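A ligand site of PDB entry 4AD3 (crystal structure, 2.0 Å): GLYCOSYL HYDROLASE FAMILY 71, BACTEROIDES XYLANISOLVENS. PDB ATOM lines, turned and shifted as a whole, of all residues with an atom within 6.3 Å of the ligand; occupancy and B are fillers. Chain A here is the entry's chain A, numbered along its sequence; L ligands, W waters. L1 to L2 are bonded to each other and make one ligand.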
ATOM      1  N   PHE A  44     -24.789  29.409  20.346  1.00  0.00           N
ATOM      2  CA  PHE A  44     -23.751  28.366  20.251  1.00  0.00           C
ATOM      3  C   PHE A  44     -23.265  27.909  21.641  1.00  0.00           C
ATOM      4  O   PHE A  44     -22.820  28.730  22.457  1.00  0.00           O
ATOM      5  CB  PHE A  44     -22.588  28.794  19.352  1.00  0.00           C
ATOM      6  CG  PHE A  44     -22.994  28.977  17.903  1.00  0.00           C
ATOM      7  CD1 PHE A  44     -23.455  27.897  17.153  1.00  0.00           C
ATOM      8  CD2 PHE A  44     -22.972  30.250  17.315  1.00  0.00           C
ATOM      9  CE1 PHE A  44     -23.882  28.089  15.802  1.00  0.00           C
ATOM     10  CE2 PHE A  44     -23.370  30.438  15.999  1.00  0.00           C
ATOM     11  CZ  PHE A  44     -23.834  29.344  15.247  1.00  0.00           C
ATOM     12  N   TYR A  46     -21.192  25.009  24.146  1.00  0.00           N
ATOM     13  CA  TYR A  46     -20.048  24.124  24.251  1.00  0.00           C
ATOM     14  C   TYR A  46     -20.191  23.214  25.485  1.00  0.00           C
ATOM     15  O   TYR A  46     -20.451  23.691  26.630  1.00  0.00           O
ATOM     16  CB  TYR A  46     -18.737  24.949  24.179  1.00  0.00           C
ATOM     17  CG  TYR A  46     -18.681  25.669  22.859  1.00  0.00           C
ATOM     18  CD1 TYR A  46     -19.360  26.875  22.664  1.00  0.00           C
ATOM     19  CD2 TYR A  46     -18.021  25.103  21.767  1.00  0.00           C
ATOM     20  CE1 TYR A  46     -19.376  27.499  21.436  1.00  0.00           C
ATOM     21  CE2 TYR A  46     -18.034  25.720  20.527  1.00  0.00           C
ATOM     22  CZ  TYR A  46     -18.711  26.927  20.373  1.00  0.00           C
ATOM     23  OH  TYR A  46     -18.739  27.549  19.126  1.00  0.00           O
ATOM     24  N   TRP A  48     -17.874  20.819  26.384  1.00  0.00           N
ATOM     25  CA  TRP A  48     -16.574  20.177  26.538  1.00  0.00           C
ATOM     26  C   TRP A  48     -15.837  20.463  27.883  1.00  0.00           C
ATOM     27  O   TRP A  48     -14.675  20.070  28.051  1.00  0.00           O
ATOM     28  CB  TRP A  48     -15.691  20.514  25.328  1.00  0.00           C
ATOM     29  CG  TRP A  48     -15.500  22.007  25.031  1.00  0.00           C
ATOM     30  CD1 TRP A  48     -15.547  23.056  25.916  1.00  0.00           C
ATOM     31  CD2 TRP A  48     -15.190  22.585  23.753  1.00  0.00           C
ATOM     32  NE1 TRP A  48     -15.289  24.237  25.278  1.00  0.00           N
ATOM     33  CE2 TRP A  48     -15.070  23.980  23.949  1.00  0.00           C
ATOM     34  CE3 TRP A  48     -14.975  22.047  22.463  1.00  0.00           C
ATOM     35  CZ2 TRP A  48     -14.751  24.865  22.893  1.00  0.00           C
ATOM     36  CZ3 TRP A  48     -14.653  22.946  21.409  1.00  0.00           C
ATOM     37  CH2 TRP A  48     -14.534  24.330  21.644  1.00  0.00           C
ATOM     38  N   HIS A  60     -10.717  21.418  29.200  1.00  0.00           N
ATOM     39  CA  HIS A  60     -10.902  22.727  28.576  1.00  0.00           C
ATOM     40  C   HIS A  60     -10.560  23.962  29.414  1.00  0.00           C
ATOM     41  O   HIS A  60     -10.013  24.919  28.882  1.00  0.00           O
ATOM     42  CB  HIS A  60     -12.237  22.846  27.821  1.00  0.00           C
ATOM     43  CG  HIS A  60     -12.138  22.340  26.414  1.00  0.00           C
ATOM     44  ND1 HIS A  60     -11.999  23.168  25.332  1.00  0.00           N
ATOM     45  CD2 HIS A  60     -12.098  21.066  25.928  1.00  0.00           C
ATOM     46  CE1 HIS A  60     -11.884  22.442  24.228  1.00  0.00           C
ATOM     47  NE2 HIS A  60     -11.954  21.172  24.567  1.00  0.00           N
ATOM     48  N   HIS A  63      -5.826  23.901  28.874  1.00  0.00           N
ATOM     49  CA  HIS A  63      -5.838  23.995  27.418  1.00  0.00           C
ATOM     50  C   HIS A  63      -4.452  24.320  26.913  1.00  0.00           C
ATOM     51  O   HIS A  63      -3.725  25.106  27.535  1.00  0.00           O
ATOM     52  CB  HIS A  63      -6.800  25.124  26.986  1.00  0.00           C
ATOM     53  CG  HIS A  63      -7.294  25.009  25.580  1.00  0.00           C
ATOM     54  ND1 HIS A  63      -6.539  25.391  24.485  1.00  0.00           N
ATOM     55  CD2 HIS A  63      -8.492  24.609  25.078  1.00  0.00           C
ATOM     56  CE1 HIS A  63      -7.249  25.225  23.379  1.00  0.00           C
ATOM     57  NE2 HIS A  63      -8.431  24.750  23.708  1.00  0.00           N
ATOM     58  N   THR A 124     -22.174  22.130  20.030  1.00  0.00           N
ATOM     59  CA  THR A 124     -20.925  21.729  19.376  1.00  0.00           C
ATOM     60  C   THR A 124     -20.888  20.200  19.274  1.00  0.00           C
ATOM     61  O   THR A 124     -21.284  19.506  20.210  1.00  0.00           O
ATOM     62  CB  THR A 124     -19.679  22.240  20.154  1.00  0.00           C
ATOM     63  OG1 THR A 124     -18.522  22.122  19.325  1.00  0.00           O
ATOM     64  CG2 THR A 124     -19.460  21.446  21.451  1.00  0.00           C
ATOM     65  N   TRP A 126     -18.421  16.921  17.882  1.00  0.00           N
ATOM     66  CA  TRP A 126     -17.058  16.559  17.439  1.00  0.00           C
ATOM     67  C   TRP A 126     -16.877  15.085  17.070  1.00  0.00           C
ATOM     68  O   TRP A 126     -15.745  14.652  16.877  1.00  0.00           O
ATOM     69  CB  TRP A 126     -16.029  16.894  18.530  1.00  0.00           C
ATOM     70  CG  TRP A 126     -15.846  18.365  18.643  1.00  0.00           C
ATOM     71  CD1 TRP A 126     -16.495  19.211  19.498  1.00  0.00           C
ATOM     72  CD2 TRP A 126     -15.001  19.177  17.824  1.00  0.00           C
ATOM     73  NE1 TRP A 126     -16.102  20.498  19.264  1.00  0.00           N
ATOM     74  CE2 TRP A 126     -15.181  20.512  18.254  1.00  0.00           C
ATOM     75  CE3 TRP A 126     -14.102  18.908  16.774  1.00  0.00           C
ATOM     76  CZ2 TRP A 126     -14.497  21.582  17.672  1.00  0.00           C
ATOM     77  CZ3 TRP A 126     -13.408  19.967  16.209  1.00  0.00           C
ATOM     78  CH2 TRP A 126     -13.607  21.296  16.662  1.00  0.00           C
ATOM     79  N   HIS A 154     -24.245  21.595  15.894  1.00  0.00           N
ATOM     80  CA  HIS A 154     -23.228  22.386  15.235  1.00  0.00           C
ATOM     81  C   HIS A 154     -22.111  21.423  14.858  1.00  0.00           C
ATOM     82  O   HIS A 154     -21.299  21.033  15.702  1.00  0.00           O
ATOM     83  CB  HIS A 154     -22.725  23.468  16.204  1.00  0.00           C
ATOM     84  CG  HIS A 154     -21.881  24.544  15.571  1.00  0.00           C
ATOM     85  ND1 HIS A 154     -21.192  25.477  16.317  1.00  0.00           N
ATOM     86  CD2 HIS A 154     -21.647  24.849  14.265  1.00  0.00           C
ATOM     87  CE1 HIS A 154     -20.564  26.309  15.502  1.00  0.00           C
ATOM     88  NE2 HIS A 154     -20.821  25.946  14.258  1.00  0.00           N
ATOM     89  N   GLU A 156     -18.826  20.198  13.714  1.00  0.00           N
ATOM     90  CA  GLU A 156     -17.491  20.777  13.712  1.00  0.00           C
ATOM     91  C   GLU A 156     -16.585  20.017  12.739  1.00  0.00           C
ATOM     92  O   GLU A 156     -16.952  18.914  12.327  1.00  0.00           O
ATOM     93  CB  GLU A 156     -16.924  20.656  15.130  1.00  0.00           C
ATOM     94  CG  GLU A 156     -17.764  21.400  16.181  1.00  0.00           C
ATOM     95  CD  GLU A 156     -17.438  22.889  16.290  1.00  0.00           C
ATOM     96  OE1 GLU A 156     -16.646  23.416  15.457  1.00  0.00           O
ATOM     97  OE2 GLU A 156     -17.959  23.536  17.234  1.00  0.00           O
ATOM     98  N   PRO A 157     -15.421  20.605  12.359  1.00  0.00           N
ATOM     99  CA  PRO A 157     -14.443  19.932  11.498  1.00  0.00           C
ATOM    100  C   PRO A 157     -13.737  18.817  12.259  1.00  0.00           C
ATOM    101  O   PRO A 157     -12.556  18.927  12.585  1.00  0.00           O
ATOM    102  CB  PRO A 157     -13.452  21.039  11.131  1.00  0.00           C
ATOM    103  CG  PRO A 157     -13.603  22.086  12.179  1.00  0.00           C
ATOM    104  CD  PRO A 157     -14.992  21.958  12.757  1.00  0.00           C
ATOM    105  N   TYR A 195     -19.712  24.000  10.586  1.00  0.00           N
ATOM    106  CA  TYR A 195     -18.586  24.909  10.800  1.00  0.00           C
ATOM    107  C   TYR A 195     -17.438  24.602   9.840  1.00  0.00           C
ATOM    108  O   TYR A 195     -17.173  23.430   9.544  1.00  0.00           O
ATOM    109  CB  TYR A 195     -18.116  24.922  12.257  1.00  0.00           C
ATOM    110  CG  TYR A 195     -17.029  25.962  12.479  1.00  0.00           C
ATOM    111  CD1 TYR A 195     -17.336  27.327  12.381  1.00  0.00           C
ATOM    112  CD2 TYR A 195     -15.699  25.593  12.680  1.00  0.00           C
ATOM    113  CE1 TYR A 195     -16.351  28.296  12.539  1.00  0.00           C
ATOM    114  CE2 TYR A 195     -14.709  26.554  12.835  1.00  0.00           C
ATOM    115  CZ  TYR A 195     -15.043  27.892  12.770  1.00  0.00           C
ATOM    116  OH  TYR A 195     -14.066  28.847  12.875  1.00  0.00           O
ATOM    117  N   ASP A 196     -16.775  25.665   9.364  1.00  0.00           N
ATOM    118  CA  ASP A 196     -15.680  25.548   8.393  1.00  0.00           C
ATOM    119  C   ASP A 196     -16.059  24.666   7.204  1.00  0.00           C
ATOM    120  O   ASP A 196     -15.273  23.794   6.752  1.00  0.00           O
ATOM    121  CB  ASP A 196     -14.396  25.019   9.062  1.00  0.00           C
ATOM    122  CG  ASP A 196     -13.658  26.099   9.831  1.00  0.00           C
ATOM    123  OD1 ASP A 196     -14.080  27.281   9.778  1.00  0.00           O
ATOM    124  OD2 ASP A 196     -12.656  25.765  10.513  1.00  0.00           O
ATOM    125  N   TYR A 250     -24.445  31.105   7.676  1.00  0.00           N
ATOM    126  CA  TYR A 250     -24.217  31.855   8.904  1.00  0.00           C
ATOM    127  C   TYR A 250     -22.797  32.355   8.853  1.00  0.00           C
ATOM    128  O   TYR A 250     -22.057  31.998   7.933  1.00  0.00           O
ATOM    129  CB  TYR A 250     -24.515  31.021  10.170  1.00  0.00           C
ATOM    130  CG  TYR A 250     -23.499  29.955  10.590  1.00  0.00           C
ATOM    131  CD1 TYR A 250     -23.153  28.909   9.721  1.00  0.00           C
ATOM    132  CD2 TYR A 250     -22.930  29.957  11.872  1.00  0.00           C
ATOM    133  CE1 TYR A 250     -22.269  27.928  10.097  1.00  0.00           C
ATOM    134  CE2 TYR A 250     -22.037  28.949  12.284  1.00  0.00           C
ATOM    135  CZ  TYR A 250     -21.713  27.949  11.374  1.00  0.00           C
ATOM    136  OH  TYR A 250     -20.836  26.937  11.716  1.00  0.00           O
ATOM    137  N   TYR A 252     -20.807  33.082  11.902  1.00  0.00           N
ATOM    138  CA  TYR A 252     -20.123  32.669  13.148  1.00  0.00           C
ATOM    139  C   TYR A 252     -19.330  33.725  13.954  1.00  0.00           C
ATOM    140  O   TYR A 252     -19.639  33.934  15.118  1.00  0.00           O
ATOM    141  CB  TYR A 252     -19.263  31.380  13.007  1.00  0.00           C
ATOM    142  CG  TYR A 252     -18.798  30.967  14.367  1.00  0.00           C
ATOM    143  CD1 TYR A 252     -19.665  30.327  15.258  1.00  0.00           C
ATOM    144  CD2 TYR A 252     -17.516  31.308  14.833  1.00  0.00           C
ATOM    145  CE1 TYR A 252     -19.272  29.997  16.552  1.00  0.00           C
ATOM    146  CE2 TYR A 252     -17.117  30.970  16.125  1.00  0.00           C
ATOM    147  CZ  TYR A 252     -17.993  30.336  16.977  1.00  0.00           C
ATOM    148  OH  TYR A 252     -17.612  30.023  18.266  1.00  0.00           O
ATOM    149  N   ASP A 291      -9.142  36.188  22.764  1.00  0.00           N
ATOM    150  CA  ASP A 291      -8.670  34.820  22.943  1.00  0.00           C
ATOM    151  C   ASP A 291      -7.178  34.763  23.223  1.00  0.00           C
ATOM    152  O   ASP A 291      -6.526  33.767  22.911  1.00  0.00           O
ATOM    153  CB  ASP A 291      -8.995  33.993  21.680  1.00  0.00           C
ATOM    154  CG  ASP A 291      -8.230  34.470  20.443  1.00  0.00           C
ATOM    155  OD1 ASP A 291      -7.409  35.420  20.517  1.00  0.00           O
ATOM    156  OD2 ASP A 291      -8.453  33.876  19.363  1.00  0.00           O
ATOM    157  N   ILE A 294      -5.163  31.821  25.176  1.00  0.00           N
ATOM    158  CA  ILE A 294      -4.809  30.648  24.388  1.00  0.00           C
ATOM    159  C   ILE A 294      -4.135  30.994  23.066  1.00  0.00           C
ATOM    160  O   ILE A 294      -3.465  30.134  22.483  1.00  0.00           O
ATOM    161  CB  ILE A 294      -6.008  29.676  24.106  1.00  0.00           C
ATOM    162  CG1 ILE A 294      -7.156  30.371  23.365  1.00  0.00           C
ATOM    163  CG2 ILE A 294      -6.464  28.976  25.403  1.00  0.00           C
ATOM    164  CD1 ILE A 294      -8.000  29.348  22.501  1.00  0.00           C
ATOM    165  N   ARG A 295      -4.311  32.218  22.591  1.00  0.00           N
ATOM    166  CA  ARG A 295      -3.673  32.666  21.343  1.00  0.00           C
ATOM    167  C   ARG A 295      -3.013  34.029  21.574  1.00  0.00           C
ATOM    168  O   ARG A 295      -3.540  35.061  21.127  1.00  0.00           O
ATOM    169  CB  ARG A 295      -4.680  32.722  20.165  1.00  0.00           C
ATOM    170  CG  ARG A 295      -5.441  31.400  19.909  1.00  0.00           C
ATOM    171  CD  ARG A 295      -6.237  31.409  18.590  1.00  0.00           C
ATOM    172  NE  ARG A 295      -7.038  30.191  18.523  1.00  0.00           N
ATOM    173  CZ  ARG A 295      -8.340  30.095  18.831  1.00  0.00           C
ATOM    174  NH1 ARG A 295      -9.035  31.166  19.215  1.00  0.00           N
ATOM    175  NH2 ARG A 295      -8.957  28.908  18.763  1.00  0.00           N
ATOM    176  N   GLU A 333     -18.382  29.916  24.838  1.00  0.00           N
ATOM    177  CA  GLU A 333     -17.045  29.761  24.288  1.00  0.00           C
ATOM    178  C   GLU A 333     -16.104  30.667  25.094  1.00  0.00           C
ATOM    179  O   GLU A 333     -15.728  31.769  24.658  1.00  0.00           O
ATOM    180  CB  GLU A 333     -16.996  30.066  22.781  1.00  0.00           C
ATOM    181  CG  GLU A 333     -16.098  29.097  21.930  1.00  0.00           C
ATOM    182  CD  GLU A 333     -14.653  28.938  22.421  1.00  0.00           C
ATOM    183  OE1 GLU A 333     -14.281  29.517  23.460  1.00  0.00           O
ATOM    184  OE2 GLU A 333     -13.860  28.211  21.773  1.00  0.00           O
ATOM    185  N   HIS A 335     -12.955  30.313  25.885  1.00  0.00           N
ATOM    186  CA  HIS A 335     -11.617  30.518  25.309  1.00  0.00           C
ATOM    187  C   HIS A 335     -11.531  31.744  24.423  1.00  0.00           C
ATOM    188  O   HIS A 335     -10.473  32.368  24.327  1.00  0.00           O
ATOM    189  CB  HIS A 335     -11.133  29.273  24.505  1.00  0.00           C
ATOM    190  CG  HIS A 335     -11.317  27.992  25.236  1.00  0.00           C
ATOM    191  ND1 HIS A 335     -11.988  26.914  24.702  1.00  0.00           N
ATOM    192  CD2 HIS A 335     -10.936  27.618  26.485  1.00  0.00           C
ATOM    193  CE1 HIS A 335     -12.018  25.931  25.584  1.00  0.00           C
ATOM    194  NE2 HIS A 335     -11.383  26.335  26.668  1.00  0.00           N
ATOM    195  N   GLU A 336     -12.645  32.092  23.785  1.00  0.00           N
ATOM    196  CA  GLU A 336     -12.632  33.178  22.799  1.00  0.00           C
ATOM    197  C   GLU A 336     -13.241  34.463  23.304  1.00  0.00           C
ATOM    198  O   GLU A 336     -13.281  35.466  22.582  1.00  0.00           O
ATOM    199  CB  GLU A 336     -13.266  32.721  21.469  1.00  0.00           C
ATOM    200  CG  GLU A 336     -12.325  31.745  20.784  1.00  0.00           C
ATOM    201  CD  GLU A 336     -12.756  31.283  19.414  1.00  0.00           C
ATOM    202  OE1 GLU A 336     -13.907  31.623  18.978  1.00  0.00           O
ATOM    203  OE2 GLU A 336     -11.920  30.549  18.798  1.00  0.00           O
HETATM  204  C1  LIG L   1     -11.289  25.510  18.020  1.00  0.00           C
HETATM  205  C2  LIG L   1     -10.567  24.165  18.206  1.00  0.00           C
HETATM  206  C3  LIG L   1     -10.762  23.669  19.629  1.00  0.00           C
HETATM  207  C4  LIG L   1     -10.296  24.704  20.639  1.00  0.00           C
HETATM  208  C5  LIG L   1     -11.027  26.016  20.378  1.00  0.00           C
HETATM  209  C6  LIG L   1     -10.567  27.108  21.346  1.00  0.00           C
HETATM  210  O1  LIG L   1     -11.125  23.216  17.330  1.00  0.00           O
HETATM  211  O2  LIG L   1     -10.044  22.477  19.819  1.00  0.00           O
HETATM  212  O3  LIG L   1     -10.608  24.221  21.922  1.00  0.00           O
HETATM  213  O4  LIG L   1     -10.809  26.412  19.017  1.00  0.00           O
HETATM  214  O5  LIG L   1     -11.289  28.308  21.159  1.00  0.00           O
HETATM  215  C1  LG2 L   2     -14.767  25.821  16.987  1.00  0.00           C
HETATM  216  O1  LG2 L   2     -14.533  24.849  15.945  1.00  0.00           O
HETATM  217  C2  LG2 L   2     -13.437  26.338  17.544  1.00  0.00           C
HETATM  218  O2  LG2 L   2     -12.698  25.233  18.083  1.00  0.00           O
HETATM  219  C3  LG2 L   2     -13.657  27.436  18.603  1.00  0.00           C
HETATM  220  O3  LG2 L   2     -14.441  26.894  19.679  1.00  0.00           O
HETATM  221  C4  LG2 L   2     -14.464  28.582  18.021  1.00  0.00           C
HETATM  222  N1  LG2 L   2     -15.710  28.006  17.563  1.00  0.00           N
HETATM  223  C5  LG2 L   2     -15.621  26.997  16.502  1.00  0.00           C
HETATM  224  C6  LG2 L   2     -17.016  26.624  16.021  1.00  0.00           C
HETATM  225  O4  LG2 L   2     -17.777  26.049  17.098  1.00  0.00           O
HETATM  226  O   HOH W   1     -10.137  20.068  17.563  1.00  0.00           O
HETATM  227  O   HOH W   2     -13.798  29.943  15.221  1.00  0.00           O
HETATM  228  O   HOH W   3     -12.040  19.974  20.295  1.00  0.00           O
HETATM  229  O   HOH W   4     -12.264  24.349  14.955  1.00  0.00           O
HETATM  230  O   HOH W   5      -7.344  22.859  19.523  1.00  0.00           O
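The side-chain carboxylate (OE1) of Glu 333 is in hydrogen-bond range of the backbone NH (N) of Glu 336. The side-chain carboxylate of Glu 333 is in hydrogen-bond range of the backbone NH of His 335, 2.9 Å away. The side-chain carboxylate (OE2) of Glu 336 is in salt-bridge range of the guanidinium group (NH1) of Arg 295. The guanidinium group (NH1) of Arg 295 is in salt-bridge range of the side-chain carboxylate (OD2) of Asp 291, 2.8 Å away. A ring nitrogen (ND1) of His 60 sits at hydrogen-bond distance from the indole nitrogen (NE1) of Trp 48, at 3.5 Å. O of His 60 lies within hydrogen-bond range of NE2 of His 335. The indole nitrogen (NE1) of Trp 126 lies within hydrogen-bond range of the side-chain hydroxyl (OG1) of Thr 124 (2.9 Å). The side-chain hydroxyl (OH) of Tyr 195 lies close to the side-chain carboxylate (OD1) of Asp 196, at 3.5 Å.
The side-chain carboxylate (OE2) of Glu 156 lies within hydrogen-bond range of an oxygen (O4) of LG2 L2, 2.5 Å away. The side-chain carboxylate (OE2) of Glu 333 is in hydrogen-bond range of an oxygen (O3) of LG2 L2 (2.5 Å). An oxygen (O4) of LG2 L2 sits at hydrogen-bond distance from the side-chain hydroxyl of Tyr 46 (2.7 Å). N1 of LG2 L2 lies within hydrogen-bond range of OH of Tyr 252, at 2.9 Å. O3 of LIG L1 is in hydrogen-bond range of NE2 of His 63 (2.9 Å). An oxygen (O4) of LIG L1 is in hydrogen-bond range of the guanidinium group of Arg 295 (3.1 Å). The side-chain carboxylate of Glu 336 sits close to an oxygen (O5) of LIG L1, 3.3 Å away.
Residues that only touch the ligand: Trp 48, His 60, Trp 126, His 154, Tyr 195, Ile 294 and His 335. Hydrophobic or aromatic side chains that line the ligand: Tyr 46, Trp 48, His 60, His 63, Trp 126, His 154, Tyr 195, Tyr 252, Ile 294 and His 335. The nearest printed residue that does not touch the ligand is Pro 157 (4.3 Å).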
